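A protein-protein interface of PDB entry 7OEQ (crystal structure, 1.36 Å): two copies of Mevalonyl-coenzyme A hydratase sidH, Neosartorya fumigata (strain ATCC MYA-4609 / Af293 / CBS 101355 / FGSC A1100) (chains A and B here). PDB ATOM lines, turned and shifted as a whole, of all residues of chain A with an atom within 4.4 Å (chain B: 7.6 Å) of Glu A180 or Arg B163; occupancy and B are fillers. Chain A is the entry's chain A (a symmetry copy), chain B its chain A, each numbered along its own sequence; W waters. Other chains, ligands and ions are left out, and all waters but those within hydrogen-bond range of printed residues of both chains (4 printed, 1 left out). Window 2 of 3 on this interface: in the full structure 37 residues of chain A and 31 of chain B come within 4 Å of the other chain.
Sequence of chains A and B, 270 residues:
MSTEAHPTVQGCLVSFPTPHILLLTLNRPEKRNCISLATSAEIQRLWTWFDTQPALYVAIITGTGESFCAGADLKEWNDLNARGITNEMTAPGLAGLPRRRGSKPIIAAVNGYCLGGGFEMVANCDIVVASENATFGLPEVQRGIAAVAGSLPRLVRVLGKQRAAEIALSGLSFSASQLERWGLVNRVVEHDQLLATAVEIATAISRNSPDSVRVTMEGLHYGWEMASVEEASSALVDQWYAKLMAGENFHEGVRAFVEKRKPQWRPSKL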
ATOM      1  N   ALA A 176     -18.985  18.206   5.511  1.00  0.00           N
ATOM      2  CA  ALA A 176     -19.897  18.122   4.357  1.00  0.00           C
ATOM      3  C   ALA A 176     -19.712  16.783   3.641  1.00  0.00           C
ATOM      4  O   ALA A 176     -20.661  16.107   3.261  1.00  0.00           O
ATOM      5  CB  ALA A 176     -19.728  19.296   3.433  1.00  0.00           C
ATOM      6  N   SER A 177     -18.458  16.411   3.369  1.00  0.00           N
ATOM      7  CA  SER A 177     -18.210  15.143   2.653  1.00  0.00           C
ATOM      8  C   SER A 177     -18.784  13.959   3.438  1.00  0.00           C
ATOM      9  O   SER A 177     -19.331  13.052   2.787  1.00  0.00           O
ATOM     10  CB  SER A 177     -16.750  14.980   2.331  1.00  0.00           C
ATOM     11  OG  SER A 177     -16.398  16.028   1.455  1.00  0.00           O
ATOM     12  N   GLN A 178     -18.672  13.954   4.768  1.00  0.00           N
ATOM     13  CA  GLN A 178     -19.247  12.860   5.612  1.00  0.00           C
ATOM     14  C   GLN A 178     -20.784  12.862   5.475  1.00  0.00           C
ATOM     15  O   GLN A 178     -21.370  11.785   5.294  1.00  0.00           O
ATOM     16  CB  GLN A 178     -18.853  12.992   7.091  1.00  0.00           C
ATOM     17  CG  GLN A 178     -17.392  12.687   7.414  1.00  0.00           C
ATOM     18  CD  GLN A 178     -17.062  12.901   8.880  1.00  0.00           C
ATOM     19  OE1 GLN A 178     -16.875  14.028   9.358  1.00  0.00           O
ATOM     20  NE2 GLN A 178     -16.950  11.801   9.611  1.00  0.00           N
ATOM     21  N   LEU A 179     -21.400  14.028   5.547  1.00  0.00           N
ATOM     22  CA  LEU A 179     -22.885  14.063   5.514  1.00  0.00           C
ATOM     23  C   LEU A 179     -23.408  13.770   4.105  1.00  0.00           C
ATOM     24  O   LEU A 179     -24.551  13.379   3.934  1.00  0.00           O
ATOM     25  CB  LEU A 179     -23.413  15.383   6.078  1.00  0.00           C
ATOM     26  CG  LEU A 179     -23.718  15.377   7.575  1.00  0.00           C
ATOM     27  CD1 LEU A 179     -24.839  14.382   7.931  1.00  0.00           C
ATOM     28  CD2 LEU A 179     -22.447  15.060   8.369  1.00  0.00           C
ATOM     29  N   GLU A 180     -22.606  13.908   3.054  1.00  0.00           N
ATOM     30  CA  GLU A 180     -22.945  13.435   1.713  1.00  0.00           C
ATOM     31  C   GLU A 180     -22.791  11.905   1.678  1.00  0.00           C
ATOM     32  O   GLU A 180     -23.674  11.221   1.153  1.00  0.00           O
ATOM     33  CB  GLU A 180     -22.038  14.111   0.676  1.00  0.00           C
ATOM     34  CG  GLU A 180     -22.431  13.736  -0.708  1.00  0.00           C
ATOM     35  CD  GLU A 180     -21.956  12.371  -1.214  1.00  0.00           C
ATOM     36  OE1 GLU A 180     -20.880  11.895  -0.767  1.00  0.00           O
ATOM     37  OE2 GLU A 180     -22.663  11.756  -2.079  1.00  0.00           O
ATOM     38  N   ARG A 181     -21.699  11.333   2.188  1.00  0.00           N
ATOM     39  CA  ARG A 181     -21.537   9.861   2.137  1.00  0.00           C
ATOM     40  C   ARG A 181     -22.690   9.234   2.936  1.00  0.00           C
ATOM     41  O   ARG A 181     -23.103   8.102   2.573  1.00  0.00           O
ATOM     42  CB  ARG A 181     -20.174   9.397   2.673  1.00  0.00           C
ATOM     43  CG  ARG A 181     -19.005   9.683   1.743  1.00  0.00           C
ATOM     44  CD  ARG A 181     -17.722   9.019   2.251  1.00  0.00           C
ATOM     45  NE  ARG A 181     -17.164   9.755   3.379  1.00  0.00           N
ATOM     46  CZ  ARG A 181     -16.360  10.806   3.251  1.00  0.00           C
ATOM     47  NH1 ARG A 181     -15.995  11.205   2.044  1.00  0.00           N
ATOM     48  NH2 ARG A 181     -15.925  11.451   4.313  1.00  0.00           N
ATOM     49  N   TRP A 182     -23.121   9.937   3.978  1.00  0.00           N
ATOM     50  CA  TRP A 182     -24.146   9.356   4.894  1.00  0.00           C
ATOM     51  C   TRP A 182     -25.588   9.630   4.452  1.00  0.00           C
ATOM     52  O   TRP A 182     -26.498   9.027   5.088  1.00  0.00           O
ATOM     53  CB  TRP A 182     -23.864   9.824   6.318  1.00  0.00           C
ATOM     54  CG  TRP A 182     -22.633   9.215   6.908  1.00  0.00           C
ATOM     55  CD1 TRP A 182     -21.818   8.275   6.343  1.00  0.00           C
ATOM     56  CD2 TRP A 182     -22.140   9.402   8.238  1.00  0.00           C
ATOM     57  NE1 TRP A 182     -20.829   7.902   7.218  1.00  0.00           N
ATOM     58  CE2 TRP A 182     -21.023   8.559   8.411  1.00  0.00           C
ATOM     59  CE3 TRP A 182     -22.538  10.197   9.316  1.00  0.00           C
ATOM     60  CZ2 TRP A 182     -20.331   8.484   9.620  1.00  0.00           C
ATOM     61  CZ3 TRP A 182     -21.849  10.122  10.506  1.00  0.00           C
ATOM     62  CH2 TRP A 182     -20.753   9.289  10.656  1.00  0.00           C
ATOM     63  N   GLY A 183     -25.839  10.472   3.475  1.00  0.00           N
ATOM     64  CA  GLY A 183     -27.189  10.513   2.865  1.00  0.00           C
ATOM     65  C   GLY A 183     -27.949  11.815   2.960  1.00  0.00           C
ATOM     66  O   GLY A 183     -28.947  11.950   2.214  1.00  0.00           O
ATOM     67  N   VAL A 185     -26.727  15.183   2.532  1.00  0.00           N
ATOM     68  CA  VAL A 185     -26.304  16.238   1.584  1.00  0.00           C
ATOM     69  C   VAL A 185     -26.360  15.653   0.156  1.00  0.00           C
ATOM     70  O   VAL A 185     -25.708  14.615  -0.100  1.00  0.00           O
ATOM     71  CB  VAL A 185     -24.893  16.736   1.953  1.00  0.00           C
ATOM     72  CG1 VAL A 185     -24.309  17.604   0.844  1.00  0.00           C
ATOM     73  CG2 VAL A 185     -24.876  17.497   3.275  1.00  0.00           C
ATOM     74  N   ASN A 186     -27.169  16.241  -0.718  1.00  0.00           N
ATOM     75  CA  ASN A 186     -27.381  15.782  -2.095  1.00  0.00           C
ATOM     76  C   ASN A 186     -26.058  15.939  -2.900  1.00  0.00           C
ATOM     77  O   ASN A 186     -25.838  15.122  -3.748  1.00  0.00           O
ATOM     78  CB  ASN A 186     -28.525  16.545  -2.753  1.00  0.00           C
ATOM     79  CG  ASN A 186     -29.904  16.253  -2.162  1.00  0.00           C
ATOM     80  OD1 ASN A 186     -30.143  16.585  -0.998  1.00  0.00           O
ATOM     81  ND2 ASN A 186     -30.724  15.649  -2.979  1.00  0.00           N
ATOM     82  N   VAL A 188     -21.973  18.033  -2.782  1.00  0.00           N
ATOM     83  CA  VAL A 188     -20.949  18.934  -2.204  1.00  0.00           C
ATOM     84  C   VAL A 188     -20.261  19.629  -3.378  1.00  0.00           C
ATOM     85  O   VAL A 188     -19.894  18.923  -4.348  1.00  0.00           O
ATOM     86  CB  VAL A 188     -19.933  18.176  -1.342  1.00  0.00           C
ATOM     87  CG1 VAL A 188     -18.853  19.125  -0.816  1.00  0.00           C
ATOM     88  CG2 VAL A 188     -20.606  17.425  -0.228  1.00  0.00           C
ATOM     89  N   LEU B 155     -39.183   5.087  -2.401  1.00  0.00           N
ATOM     90  CA  LEU B 155     -37.886   5.770  -2.673  1.00  0.00           C
ATOM     91  C   LEU B 155     -37.460   6.565  -1.452  1.00  0.00           C
ATOM     92  O   LEU B 155     -36.267   6.643  -1.139  1.00  0.00           O
ATOM     93  CB  LEU B 155     -37.995   6.654  -3.915  1.00  0.00           C
ATOM     94  CG  LEU B 155     -38.062   5.898  -5.244  1.00  0.00           C
ATOM     95  CD1 LEU B 155     -38.370   6.849  -6.401  1.00  0.00           C
ATOM     96  CD2 LEU B 155     -36.800   5.110  -5.501  1.00  0.00           C
ATOM     97  N   VAL B 156     -38.412   7.183  -0.726  1.00  0.00           N
ATOM     98  CA  VAL B 156     -38.073   7.899   0.535  1.00  0.00           C
ATOM     99  C   VAL B 156     -37.369   6.917   1.475  1.00  0.00           C
ATOM    100  O   VAL B 156     -36.390   7.300   2.139  1.00  0.00           O
ATOM    101  CB  VAL B 156     -39.328   8.544   1.183  1.00  0.00           C
ATOM    102  CG1 VAL B 156     -39.085   8.993   2.614  1.00  0.00           C
ATOM    103  CG2 VAL B 156     -39.758   9.715   0.322  1.00  0.00           C
ATOM    104  N   VAL B 158     -35.746   4.053   0.749  1.00  0.00           N
ATOM    105  CA  VAL B 158     -34.449   3.518   0.220  1.00  0.00           C
ATOM    106  C   VAL B 158     -33.393   4.614   0.072  1.00  0.00           C
ATOM    107  O   VAL B 158     -32.231   4.374   0.485  1.00  0.00           O
ATOM    108  CB  VAL B 158     -34.700   2.770  -1.083  1.00  0.00           C
ATOM    109  CG1 VAL B 158     -33.373   2.327  -1.684  1.00  0.00           C
ATOM    110  CG2 VAL B 158     -35.606   1.568  -0.837  1.00  0.00           C
ATOM    111  N   LEU B 159     -33.744   5.712  -0.562  1.00  0.00           N
ATOM    112  CA  LEU B 159     -32.750   6.758  -0.901  1.00  0.00           C
ATOM    113  C   LEU B 159     -32.602   7.769   0.231  1.00  0.00           C
ATOM    114  O   LEU B 159     -31.628   8.521   0.249  1.00  0.00           O
ATOM    115  CB  LEU B 159     -33.189   7.497  -2.153  1.00  0.00           C
ATOM    116  CG  LEU B 159     -33.443   6.662  -3.393  1.00  0.00           C
ATOM    117  CD1 LEU B 159     -33.826   7.579  -4.541  1.00  0.00           C
ATOM    118  CD2 LEU B 159     -32.243   5.802  -3.775  1.00  0.00           C
ATOM    119  N   GLY B 160     -33.606   7.867   1.091  1.00  0.00           N
ATOM    120  CA  GLY B 160     -33.780   8.998   2.002  1.00  0.00           C
ATOM    121  C   GLY B 160     -34.614  10.105   1.374  1.00  0.00           C
ATOM    122  O   GLY B 160     -34.679  10.212   0.142  1.00  0.00           O
ATOM    123  N   LYS B 161     -35.278  10.909   2.215  1.00  0.00           N
ATOM    124  CA  LYS B 161     -36.220  11.945   1.728  1.00  0.00           C
ATOM    125  C   LYS B 161     -35.549  12.868   0.700  1.00  0.00           C
ATOM    126  O   LYS B 161     -36.177  13.159  -0.322  1.00  0.00           O
ATOM    127  CB  LYS B 161     -36.740  12.756   2.908  1.00  0.00           C
ATOM    128  CG  LYS B 161     -37.522  14.014   2.568  1.00  0.00           C
ATOM    129  CD  LYS B 161     -37.817  14.791   3.856  1.00  0.00           C
ATOM    130  CE  LYS B 161     -38.025  16.284   3.687  1.00  0.00           C
ATOM    131  NZ  LYS B 161     -39.422  16.527   3.290  1.00  0.00           N
ATOM    132  N   GLN B 162     -34.331  13.350   1.018  1.00  0.00           N
ATOM    133  CA  GLN B 162     -33.764  14.474   0.203  1.00  0.00           C
ATOM    134  C   GLN B 162     -33.373  13.986  -1.231  1.00  0.00           C
ATOM    135  O   GLN B 162     -33.538  14.757  -2.191  1.00  0.00           O
ATOM    136  CB  GLN B 162     -32.521  15.049   0.879  1.00  0.00           C
ATOM    137  CG  GLN B 162     -32.818  15.904   2.117  1.00  0.00           C
ATOM    138  CD  GLN B 162     -33.179  15.145   3.372  1.00  0.00           C
ATOM    139  OE1 GLN B 162     -32.941  13.942   3.498  1.00  0.00           O
ATOM    140  NE2 GLN B 162     -33.671  15.907   4.348  1.00  0.00           N
ATOM    141  N   ARG B 163     -32.941  12.737  -1.348  1.00  0.00           N
ATOM    142  CA  ARG B 163     -32.585  12.162  -2.660  1.00  0.00           C
ATOM    143  C   ARG B 163     -33.824  11.768  -3.446  1.00  0.00           C
ATOM    144  O   ARG B 163     -33.878  12.040  -4.660  1.00  0.00           O
ATOM    145  CB  ARG B 163     -31.549  11.063  -2.458  1.00  0.00           C
ATOM    146  CG  ARG B 163     -30.218  11.675  -2.101  1.00  0.00           C
ATOM    147  CD  ARG B 163     -29.240  10.749  -1.433  1.00  0.00           C
ATOM    148  NE  ARG B 163     -28.114  11.521  -1.033  1.00  0.00           N
ATOM    149  CZ  ARG B 163     -26.986  11.002  -0.606  1.00  0.00           C
ATOM    150  NH1 ARG B 163     -26.875   9.686  -0.514  1.00  0.00           N
ATOM    151  NH2 ARG B 163     -25.972  11.806  -0.332  1.00  0.00           N
ATOM    152  N   ALA B 164     -34.824  11.186  -2.772  1.00  0.00           N
ATOM    153  CA  ALA B 164     -36.118  10.933  -3.439  1.00  0.00           C
ATOM    154  C   ALA B 164     -36.694  12.268  -3.953  1.00  0.00           C
ATOM    155  O   ALA B 164     -37.217  12.314  -5.074  1.00  0.00           O
ATOM    156  CB  ALA B 164     -37.073  10.281  -2.455  1.00  0.00           C
ATOM    157  N   ALA B 165     -36.610  13.319  -3.137  1.00  0.00           N
ATOM    158  CA  ALA B 165     -37.108  14.663  -3.503  1.00  0.00           C
ATOM    159  C   ALA B 165     -36.380  15.211  -4.728  1.00  0.00           C
ATOM    160  O   ALA B 165     -37.035  15.702  -5.663  1.00  0.00           O
ATOM    161  CB  ALA B 165     -37.033  15.619  -2.332  1.00  0.00           C
ATOM    162  N   GLU B 166     -35.051  15.101  -4.743  1.00  0.00           N
ATOM    163  CA  GLU B 166     -34.318  15.673  -5.894  1.00  0.00           C
ATOM    164  C   GLU B 166     -34.745  14.954  -7.187  1.00  0.00           C
ATOM    165  O   GLU B 166     -35.066  15.624  -8.191  1.00  0.00           O
ATOM    166  CB  GLU B 166     -32.824  15.581  -5.664  1.00  0.00           C
ATOM    167  CG  GLU B 166     -32.095  16.191  -6.841  1.00  0.00           C
ATOM    168  CD  GLU B 166     -30.575  16.156  -6.793  1.00  0.00           C
ATOM    169  OE1 GLU B 166     -30.004  15.676  -5.782  1.00  0.00           O
ATOM    170  OE2 GLU B 166     -29.950  16.553  -7.818  1.00  0.00           O
ATOM    171  N   ILE B 167     -34.854  13.626  -7.146  1.00  0.00           N
ATOM    172  CA  ILE B 167     -35.246  12.863  -8.352  1.00  0.00           C
ATOM    173  C   ILE B 167     -36.687  13.243  -8.744  1.00  0.00           C
ATOM    174  O   ILE B 167     -36.941  13.603  -9.908  1.00  0.00           O
ATOM    175  CB  ILE B 167     -35.092  11.356  -8.091  1.00  0.00           C
ATOM    176  CG1 ILE B 167     -33.618  11.016  -7.897  1.00  0.00           C
ATOM    177  CG2 ILE B 167     -35.734  10.539  -9.176  1.00  0.00           C
ATOM    178  CD1 ILE B 167     -33.360   9.545  -7.659  1.00  0.00           C
ATOM    179  N   ALA B 168     -37.626  13.114  -7.794  1.00  0.00           N
ATOM    180  CA  ALA B 168     -39.051  13.215  -8.140  1.00  0.00           C
ATOM    181  C   ALA B 168     -39.448  14.660  -8.460  1.00  0.00           C
ATOM    182  O   ALA B 168     -40.302  14.851  -9.337  1.00  0.00           O
ATOM    183  CB  ALA B 168     -39.940  12.640  -7.049  1.00  0.00           C
ATOM    184  N   LEU B 169     -38.915  15.643  -7.745  1.00  0.00           N
ATOM    185  CA  LEU B 169     -39.288  17.058  -7.995  1.00  0.00           C
ATOM    186  C   LEU B 169     -38.661  17.603  -9.277  1.00  0.00           C
ATOM    187  O   LEU B 169     -39.274  18.466  -9.916  1.00  0.00           O
ATOM    188  CB  LEU B 169     -38.940  17.935  -6.793  1.00  0.00           C
ATOM    189  CG  LEU B 169     -39.633  17.558  -5.493  1.00  0.00           C
ATOM    190  CD1 LEU B 169     -38.970  18.273  -4.333  1.00  0.00           C
ATOM    191  CD2 LEU B 169     -41.143  17.875  -5.537  1.00  0.00           C
ATOM    192  N   SER B 170     -37.443  17.172  -9.607  1.00  0.00           N
ATOM    193  CA  SER B 170     -36.735  17.697 -10.796  1.00  0.00           C
ATOM    194  C   SER B 170     -37.225  17.036 -12.092  1.00  0.00           C
ATOM    195  O   SER B 170     -37.275  17.722 -13.116  1.00  0.00           O
ATOM    196  CB  SER B 170     -35.232  17.564 -10.689  1.00  0.00           C
ATOM    197  OG  SER B 170     -34.797  16.212 -10.858  1.00  0.00           O
ATOM    198  N   PHE B 174     -30.770  10.419 -13.939  1.00  0.00           N
ATOM    199  CA  PHE B 174     -29.656  10.132 -13.001  1.00  0.00           C
ATOM    200  C   PHE B 174     -28.988   8.829 -13.417  1.00  0.00           C
ATOM    201  O   PHE B 174     -29.621   7.948 -13.952  1.00  0.00           O
ATOM    202  CB  PHE B 174     -30.240  10.012 -11.595  1.00  0.00           C
ATOM    203  CG  PHE B 174     -30.802  11.310 -11.081  1.00  0.00           C
ATOM    204  CD1 PHE B 174     -32.072  11.733 -11.430  1.00  0.00           C
ATOM    205  CD2 PHE B 174     -30.026  12.149 -10.293  1.00  0.00           C
ATOM    206  CE1 PHE B 174     -32.520  12.969 -11.021  1.00  0.00           C
ATOM    207  CE2 PHE B 174     -30.494  13.383  -9.870  1.00  0.00           C
ATOM    208  CZ  PHE B 174     -31.748  13.785 -10.230  1.00  0.00           C
ATOM    209  N   GLN B 178     -24.949   6.877  -9.774  1.00  0.00           N
ATOM    210  CA  GLN B 178     -25.641   7.730  -8.755  1.00  0.00           C
ATOM    211  C   GLN B 178     -26.637   6.865  -7.955  1.00  0.00           C
ATOM    212  O   GLN B 178     -26.662   6.967  -6.720  1.00  0.00           O
ATOM    213  CB  GLN B 178     -26.373   8.922  -9.388  1.00  0.00           C
ATOM    214  CG  GLN B 178     -25.477  10.031  -9.938  1.00  0.00           C
ATOM    215  CD  GLN B 178     -26.267  11.142 -10.604  1.00  0.00           C
ATOM    216  OE1 GLN B 178     -26.733  11.028 -11.746  1.00  0.00           O
ATOM    217  NE2 GLN B 178     -26.396  12.258  -9.901  1.00  0.00           N
ATOM    218  N   LEU B 179     -27.411   6.041  -8.638  1.00  0.00           N
ATOM    219  CA  LEU B 179     -28.449   5.260  -7.915  1.00  0.00           C
ATOM    220  C   LEU B 179     -27.813   4.132  -7.098  1.00  0.00           C
ATOM    221  O   LEU B 179     -28.411   3.630  -6.160  1.00  0.00           O
ATOM    222  CB  LEU B 179     -29.526   4.758  -8.879  1.00  0.00           C
ATOM    223  CG  LEU B 179     -30.730   5.683  -9.050  1.00  0.00           C
ATOM    224  CD1 LEU B 179     -31.509   5.864  -7.733  1.00  0.00           C
ATOM    225  CD2 LEU B 179     -30.277   7.041  -9.596  1.00  0.00           C
ATOM    226  N   ARG B 181     -24.727   4.796  -5.495  1.00  0.00           N
ATOM    227  CA  ARG B 181     -24.211   5.558  -4.332  1.00  0.00           C
ATOM    228  C   ARG B 181     -25.398   5.862  -3.405  1.00  0.00           C
ATOM    229  O   ARG B 181     -25.168   5.947  -2.171  1.00  0.00           O
ATOM    230  CB  ARG B 181     -23.486   6.847  -4.746  1.00  0.00           C
ATOM    231  CG  ARG B 181     -22.116   6.624  -5.368  1.00  0.00           C
ATOM    232  CD  ARG B 181     -21.378   7.950  -5.568  1.00  0.00           C
ATOM    233  NE  ARG B 181     -21.914   8.679  -6.712  1.00  0.00           N
ATOM    234  CZ  ARG B 181     -21.524   8.475  -7.966  1.00  0.00           C
ATOM    235  NH1 ARG B 181     -20.567   7.597  -8.217  1.00  0.00           N
ATOM    236  NH2 ARG B 181     -22.080   9.140  -8.957  1.00  0.00           N
ATOM    237  N   TRP B 182     -26.569   6.051  -4.007  1.00  0.00           N
ATOM    238  CA  TRP B 182     -27.753   6.481  -3.208  1.00  0.00           C
ATOM    239  C   TRP B 182     -28.549   5.311  -2.617  1.00  0.00           C
ATOM    240  O   TRP B 182     -29.462   5.608  -1.795  1.00  0.00           O
ATOM    241  CB  TRP B 182     -28.613   7.414  -4.053  1.00  0.00           C
ATOM    242  CG  TRP B 182     -27.981   8.748  -4.292  1.00  0.00           C
ATOM    243  CD1 TRP B 182     -26.795   9.206  -3.790  1.00  0.00           C
ATOM    244  CD2 TRP B 182     -28.558   9.857  -4.988  1.00  0.00           C
ATOM    245  NE1 TRP B 182     -26.581  10.509  -4.167  1.00  0.00           N
ATOM    246  CE2 TRP B 182     -27.671  10.947  -4.881  1.00  0.00           C
ATOM    247  CE3 TRP B 182     -29.751  10.042  -5.691  1.00  0.00           C
ATOM    248  CZ2 TRP B 182     -27.963  12.196  -5.431  1.00  0.00           C
ATOM    249  CZ3 TRP B 182     -30.031  11.276  -6.234  1.00  0.00           C
ATOM    250  CH2 TRP B 182     -29.148  12.336  -6.121  1.00  0.00           C
ATOM    251  N   GLY B 183     -28.291   4.075  -2.980  1.00  0.00           N
ATOM    252  CA  GLY B 183     -28.853   2.946  -2.203  1.00  0.00           C
ATOM    253  C   GLY B 183     -29.779   2.000  -2.932  1.00  0.00           C
ATOM    254  O   GLY B 183     -30.024   0.902  -2.380  1.00  0.00           O
HETATM  255  O   HOH W   1     -29.145  13.914   0.121  1.00  0.00           O
HETATM  256  O   HOH W   2     -24.027   9.110  -0.885  1.00  0.00           O
HETATM  257  O   HOH W   3     -24.531  12.527  -3.737  1.00  0.00           O
HETATM  258  O   HOH W   4     -27.260  15.773  -6.274  1.00  0.00           O
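The backbone carbonyl oxygen (O) of Leu A179 sits at hydrogen-bond distance from the backbone NH (N) of Val A185 (3.2 Å).
O of Glu B166 lies within hydrogen-bond range of OG of Ser B170, at 2.7 Å.
Printed residues of chain A that touch a printed residue of chain B: Glu A180, Gly A183, Val A185 and Asn A186.
Of the 21 printed residues of chain B, 4 touch a printed residue of chain A.
Printed residues of chain B that touch a printed residue of chain A: Gln B162, Arg B163, Glu B166 and Trp B182.
Hydrophobic or aromatic side chains of chain B within 4 Å of the printed part of chain A: Trp B182.
Among the printed residues, 7 pairs touch across the chains.
Among the printed residues, Asp or Glu carboxylates within 4 Å of a Lys or Arg side-chain nitrogen of the other chain: Glu A180 with Arg B163 (3.7 Å).
5 positions are printed for both chains.
Water W3 lies within hydrogen-bond range of the side-chain carboxylate (OE2) of Glu A180 (2.6 Å), the backbone carbonyl oxygen (O) of Asn A186 (2.9 Å) and the indole nitrogen (NE1) of Trp B182 (2.9 Å).
Water W4 bridges the side-chain carboxylate (OE1) of Glu B166 and the backbone carbonyl oxygen (O) of Asn A186.
Water W1 lies within hydrogen-bond range of the guanidinium group of Arg B163 (2.8 Å), the backbone carbonyl oxygen of Gly A183 (2.9 Å) and the side-chain amide oxygen of Asn A186 (3.1 Å).
Water W2 bridges the guanidinium group of Arg B163 (2.9 Å) and the backbone carbonyl oxygen of Glu A180 (3.0 Å).
Of the printed residues of chain B, Glu A180 touches Arg B163.
Printed residues of chain B within 4 Å of Val A185: Arg B163.
Arg B163 touches just these residues of chain A: Glu A180, Gly A183, Val A185 and Asn A186.
Of the printed residues of chain A, Glu B166 touches Asn A186.
Ala B168 touches none of the printed residues of chain A.
The nearest printed residue of chain B that does not touch Glu A180 is Trp B182 (4.6 Å).
Among the printed residues, pairs that only touch across the chains: Asn A186 with Arg B163 and Asn A186 with Trp B182.
The guanidinium group (NH2) of Arg B163 is in salt-bridge range of the side-chain carboxylate (OE2) of Glu A180, 3.7 Å away.
The backbone carbonyl oxygen of Val A185 lies within hydrogen-bond range of the guanidinium group of Arg B163 (2.8 Å).
O of Gln B162 sits at hydrogen-bond distance from ND2 of Asn A186.
NE of Arg B163 sits at hydrogen-bond distance from O of Gly A183, 3.4 Å away.
ND2 of Asn A186 lies within hydrogen-bond range of OE1 of Glu B166 (2.9 Å).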
